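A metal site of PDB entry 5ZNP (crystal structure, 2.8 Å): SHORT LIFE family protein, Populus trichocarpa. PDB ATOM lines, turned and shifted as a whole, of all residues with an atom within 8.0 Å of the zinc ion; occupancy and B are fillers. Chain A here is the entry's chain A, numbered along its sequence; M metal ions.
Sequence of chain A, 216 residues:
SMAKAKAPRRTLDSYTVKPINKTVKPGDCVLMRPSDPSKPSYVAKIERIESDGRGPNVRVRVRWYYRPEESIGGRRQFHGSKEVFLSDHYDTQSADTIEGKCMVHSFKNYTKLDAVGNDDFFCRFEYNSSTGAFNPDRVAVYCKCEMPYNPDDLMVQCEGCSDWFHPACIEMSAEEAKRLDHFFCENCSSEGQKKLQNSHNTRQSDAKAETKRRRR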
ATOM      1  N   GLN A  77      -3.813  30.109  -0.840  1.00  0.00           N
ATOM      2  CA  GLN A  77      -3.268  30.212  -2.192  1.00  0.00           C
ATOM      3  C   GLN A  77      -4.335  30.434  -3.266  1.00  0.00           C
ATOM      4  O   GLN A  77      -4.133  31.223  -4.195  1.00  0.00           O
ATOM      5  CB  GLN A  77      -2.478  28.942  -2.519  1.00  0.00           C
ATOM      6  CG  GLN A  77      -3.230  27.663  -2.172  1.00  0.00           C
ATOM      7  CD  GLN A  77      -2.490  26.412  -2.577  1.00  0.00           C
ATOM      8  OE1 GLN A  77      -1.370  26.476  -3.083  1.00  0.00           O
ATOM      9  NE2 GLN A  77      -3.119  25.265  -2.362  1.00  0.00           N
ATOM     10  N   TYR A 142      -8.943  21.927  -9.699  1.00  0.00           N
ATOM     11  CA  TYR A 142      -8.247  21.692 -10.958  1.00  0.00           C
ATOM     12  C   TYR A 142      -6.764  21.372 -10.772  1.00  0.00           C
ATOM     13  O   TYR A 142      -6.233  21.500  -9.678  1.00  0.00           O
ATOM     14  CB  TYR A 142      -8.399  22.908 -11.879  1.00  0.00           C
ATOM     15  CG  TYR A 142      -9.824  23.396 -12.016  1.00  0.00           C
ATOM     16  CD1 TYR A 142     -10.287  24.451 -11.225  1.00  0.00           C
ATOM     17  CD2 TYR A 142     -10.699  22.805 -12.911  1.00  0.00           C
ATOM     18  CE1 TYR A 142     -11.585  24.895 -11.342  1.00  0.00           C
ATOM     19  CE2 TYR A 142     -12.011  23.251 -13.030  1.00  0.00           C
ATOM     20  CZ  TYR A 142     -12.441  24.293 -12.234  1.00  0.00           C
ATOM     21  OH  TYR A 142     -13.739  24.737 -12.351  1.00  0.00           O
ATOM     22  N   CYS A 143      -6.121  20.947 -11.858  1.00  0.00           N
ATOM     23  CA  CYS A 143      -4.689  20.629 -11.901  1.00  0.00           C
ATOM     24  C   CYS A 143      -4.303  19.494 -10.954  1.00  0.00           C
ATOM     25  O   CYS A 143      -5.169  18.886 -10.320  1.00  0.00           O
ATOM     26  CB  CYS A 143      -3.862  21.883 -11.579  1.00  0.00           C
ATOM     27  SG  CYS A 143      -2.084  21.675 -11.813  1.00  0.00           S
ATOM     28  N   LYS A 144      -3.009  19.202 -10.868  1.00  0.00           N
ATOM     29  CA  LYS A 144      -2.527  18.125 -10.007  1.00  0.00           C
ATOM     30  C   LYS A 144      -2.536  18.551  -8.550  1.00  0.00           C
ATOM     31  O   LYS A 144      -2.613  17.713  -7.643  1.00  0.00           O
ATOM     32  CB  LYS A 144      -1.122  17.691 -10.389  1.00  0.00           C
ATOM     33  CG  LYS A 144      -0.821  17.696 -11.870  1.00  0.00           C
ATOM     34  CD  LYS A 144       0.607  17.233 -12.107  1.00  0.00           C
ATOM     35  CE  LYS A 144       1.585  17.890 -11.136  1.00  0.00           C
ATOM     36  NZ  LYS A 144       1.509  19.375 -11.145  1.00  0.00           N
ATOM     37  N   CYS A 145      -2.457  19.852  -8.313  1.00  0.00           N
ATOM     38  CA  CYS A 145      -2.553  20.390  -6.970  1.00  0.00           C
ATOM     39  C   CYS A 145      -3.956  20.157  -6.428  1.00  0.00           C
ATOM     40  O   CYS A 145      -4.176  20.168  -5.217  1.00  0.00           O
ATOM     41  CB  CYS A 145      -2.209  21.887  -6.955  1.00  0.00           C
ATOM     42  SG  CYS A 145      -3.162  22.890  -8.111  1.00  0.00           S
ATOM     43  N   GLU A 146      -4.898  19.945  -7.352  1.00  0.00           N
ATOM     44  CA  GLU A 146      -6.303  19.713  -7.032  1.00  0.00           C
ATOM     45  C   GLU A 146      -6.829  20.767  -6.068  1.00  0.00           C
ATOM     46  O   GLU A 146      -7.379  20.459  -5.020  1.00  0.00           O
ATOM     47  CB  GLU A 146      -6.502  18.302  -6.469  1.00  0.00           C
ATOM     48  CG  GLU A 146      -6.242  17.203  -7.493  1.00  0.00           C
ATOM     49  CD  GLU A 146      -6.855  15.877  -7.115  1.00  0.00           C
ATOM     50  OE1 GLU A 146      -6.696  15.449  -5.948  1.00  0.00           O
ATOM     51  OE2 GLU A 146      -7.501  15.253  -7.984  1.00  0.00           O
ATOM     52  N   MET A 147      -6.620  22.020  -6.458  1.00  0.00           N
ATOM     53  CA  MET A 147      -7.043  23.176  -5.671  1.00  0.00           C
ATOM     54  C   MET A 147      -8.092  23.969  -6.437  1.00  0.00           C
ATOM     55  O   MET A 147      -8.147  23.913  -7.660  1.00  0.00           O
ATOM     56  CB  MET A 147      -5.848  24.065  -5.334  1.00  0.00           C
ATOM     57  CG  MET A 147      -4.802  23.406  -4.436  1.00  0.00           C
ATOM     58  SD  MET A 147      -5.198  23.546  -2.685  1.00  0.00           S
ATOM     59  CE  MET A 147      -5.963  21.961  -2.371  1.00  0.00           C
ATOM     60  N   PRO A 148      -8.952  24.707  -5.708  1.00  0.00           N
ATOM     61  CA  PRO A 148      -9.915  25.610  -6.339  1.00  0.00           C
ATOM     62  C   PRO A 148      -9.238  26.687  -7.184  1.00  0.00           C
ATOM     63  O   PRO A 148      -8.055  26.965  -7.002  1.00  0.00           O
ATOM     64  CB  PRO A 148     -10.653  26.235  -5.156  1.00  0.00           C
ATOM     65  CG  PRO A 148     -10.513  25.225  -4.065  1.00  0.00           C
ATOM     66  CD  PRO A 148      -9.159  24.629  -4.253  1.00  0.00           C
ATOM     67  N   LEU A 154      -2.913  32.040 -13.961  1.00  0.00           N
ATOM     68  CA  LEU A 154      -3.087  31.592 -15.334  1.00  0.00           C
ATOM     69  C   LEU A 154      -3.076  30.064 -15.427  1.00  0.00           C
ATOM     70  O   LEU A 154      -2.156  29.409 -14.933  1.00  0.00           O
ATOM     71  CB  LEU A 154      -1.984  32.166 -16.226  1.00  0.00           C
ATOM     72  CG  LEU A 154      -2.093  31.934 -17.730  1.00  0.00           C
ATOM     73  CD1 LEU A 154      -2.816  33.084 -18.406  1.00  0.00           C
ATOM     74  CD2 LEU A 154      -0.717  31.713 -18.339  1.00  0.00           C
ATOM     75  N   MET A 155      -4.109  29.514 -16.052  1.00  0.00           N
ATOM     76  CA  MET A 155      -4.174  28.075 -16.298  1.00  0.00           C
ATOM     77  C   MET A 155      -4.329  27.800 -17.789  1.00  0.00           C
ATOM     78  O   MET A 155      -4.599  28.717 -18.567  1.00  0.00           O
ATOM     79  CB  MET A 155      -5.328  27.442 -15.526  1.00  0.00           C
ATOM     80  CG  MET A 155      -5.290  27.686 -14.022  1.00  0.00           C
ATOM     81  SD  MET A 155      -6.670  26.903 -13.173  1.00  0.00           S
ATOM     82  CE  MET A 155      -5.810  25.671 -12.204  1.00  0.00           C
ATOM     83  N   TRP A 164      -7.326  21.978 -16.451  1.00  0.00           N
ATOM     84  CA  TRP A 164      -6.574  23.186 -16.546  1.00  0.00           C
ATOM     85  C   TRP A 164      -5.400  23.070 -15.617  1.00  0.00           C
ATOM     86  O   TRP A 164      -5.509  22.470 -14.563  1.00  0.00           O
ATOM     87  CB  TRP A 164      -7.446  24.359 -16.131  1.00  0.00           C
ATOM     88  CG  TRP A 164      -8.632  24.618 -17.000  1.00  0.00           C
ATOM     89  CD1 TRP A 164      -9.847  24.029 -16.915  1.00  0.00           C
ATOM     90  CD2 TRP A 164      -8.719  25.532 -18.074  1.00  0.00           C
ATOM     91  NE1 TRP A 164     -10.676  24.516 -17.861  1.00  0.00           N
ATOM     92  CE2 TRP A 164      -9.991  25.452 -18.593  1.00  0.00           C
ATOM     93  CE3 TRP A 164      -7.821  26.427 -18.632  1.00  0.00           C
ATOM     94  CZ2 TRP A 164     -10.405  26.215 -19.647  1.00  0.00           C
ATOM     95  CZ3 TRP A 164      -8.226  27.173 -19.674  1.00  0.00           C
ATOM     96  CH2 TRP A 164      -9.496  27.070 -20.183  1.00  0.00           C
ATOM     97  N   PHE A 165      -4.294  23.651 -16.002  1.00  0.00           N
ATOM     98  CA  PHE A 165      -3.098  23.500 -15.212  1.00  0.00           C
ATOM     99  C   PHE A 165      -2.348  24.783 -14.922  1.00  0.00           C
ATOM    100  O   PHE A 165      -2.193  25.607 -15.787  1.00  0.00           O
ATOM    101  CB  PHE A 165      -2.208  22.460 -15.877  1.00  0.00           C
ATOM    102  CG  PHE A 165      -2.847  21.116 -15.968  1.00  0.00           C
ATOM    103  CD1 PHE A 165      -3.858  20.886 -16.842  1.00  0.00           C
ATOM    104  CD2 PHE A 165      -2.462  20.100 -15.152  1.00  0.00           C
ATOM    105  CE1 PHE A 165      -4.467  19.673 -16.928  1.00  0.00           C
ATOM    106  CE2 PHE A 165      -3.067  18.879 -15.228  1.00  0.00           C
ATOM    107  CZ  PHE A 165      -4.074  18.662 -16.111  1.00  0.00           C
ATOM    108  N   HIS A 166      -1.867  24.951 -13.694  1.00  0.00           N
ATOM    109  CA  HIS A 166      -0.835  25.950 -13.443  1.00  0.00           C
ATOM    110  C   HIS A 166       0.450  25.466 -14.096  1.00  0.00           C
ATOM    111  O   HIS A 166       0.855  24.327 -13.885  1.00  0.00           O
ATOM    112  CB  HIS A 166      -0.623  26.179 -11.953  1.00  0.00           C
ATOM    113  CG  HIS A 166      -1.848  26.628 -11.209  1.00  0.00           C
ATOM    114  ND1 HIS A 166      -2.460  25.838 -10.263  1.00  0.00           N
ATOM    115  CD2 HIS A 166      -2.556  27.779 -11.275  1.00  0.00           C
ATOM    116  CE1 HIS A 166      -3.502  26.486  -9.774  1.00  0.00           C
ATOM    117  NE2 HIS A 166      -3.579  27.665 -10.370  1.00  0.00           N
ATOM    118  N   PRO A 167       1.097  26.332 -14.895  1.00  0.00           N
ATOM    119  CA  PRO A 167       2.373  25.978 -15.530  1.00  0.00           C
ATOM    120  C   PRO A 167       3.430  25.572 -14.508  1.00  0.00           C
ATOM    121  O   PRO A 167       4.107  24.555 -14.700  1.00  0.00           O
ATOM    122  CB  PRO A 167       2.768  27.265 -16.235  1.00  0.00           C
ATOM    123  CG  PRO A 167       1.474  27.950 -16.524  1.00  0.00           C
ATOM    124  CD  PRO A 167       0.607  27.643 -15.342  1.00  0.00           C
ATOM    125  N   ALA A 168       3.565  26.351 -13.444  1.00  0.00           N
ATOM    126  CA  ALA A 168       4.541  26.087 -12.394  1.00  0.00           C
ATOM    127  C   ALA A 168       4.332  24.726 -11.751  1.00  0.00           C
ATOM    128  O   ALA A 168       5.289  24.067 -11.323  1.00  0.00           O
ATOM    129  CB  ALA A 168       4.503  27.183 -11.345  1.00  0.00           C
ATOM    130  N   CYS A 169       3.075  24.302 -11.672  1.00  0.00           N
ATOM    131  CA  CYS A 169       2.740  22.994 -11.099  1.00  0.00           C
ATOM    132  C   CYS A 169       3.287  21.855 -11.959  1.00  0.00           C
ATOM    133  O   CYS A 169       3.493  20.742 -11.464  1.00  0.00           O
ATOM    134  CB  CYS A 169       1.223  22.850 -10.938  1.00  0.00           C
ATOM    135  SG  CYS A 169       0.517  23.810  -9.577  1.00  0.00           S
ATOM    136  N   ILE A 170       3.516  22.124 -13.238  1.00  0.00           N
ATOM    137  CA  ILE A 170       4.053  21.109 -14.129  1.00  0.00           C
ATOM    138  C   ILE A 170       5.186  21.606 -15.016  1.00  0.00           C
ATOM    139  O   ILE A 170       5.106  21.533 -16.243  1.00  0.00           O
ATOM    140  CB  ILE A 170       2.972  20.519 -15.055  1.00  0.00           C
ATOM    141  CG1 ILE A 170       2.001  21.605 -15.516  1.00  0.00           C
ATOM    142  CG2 ILE A 170       2.225  19.415 -14.353  1.00  0.00           C
ATOM    143  CD1 ILE A 170       0.860  21.059 -16.339  1.00  0.00           C
HETATM  144 ZN    ZN M   1      -1.845  23.475 -10.194  1.00  0.00          ZN
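Within 4 Å of the zinc ion: Cys 143, Cys 145, His 166 and Cys 169.
The zinc ion is bound by SG of Cys 143 (2.4 Å). The zinc ion is bound by ND1 of His 166 (2.4 Å). The zinc ion is bound by SG of Cys 169 (2.5 Å). The zinc ion is bound by the side-chain sulfur (SG) of Cys 145. The zinc ion has four donor atoms within binding distance.
The backbone carbonyl oxygen (O) of Trp 164 sits at hydrogen-bond distance from the backbone NH (N) of Cys 143 (3.2 Å). NZ of Lys 144 is in hydrogen-bond range of O of Cys 169 (2.4 Å). SG of Cys 145 sits close to O of Tyr 142 (3.7 Å).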
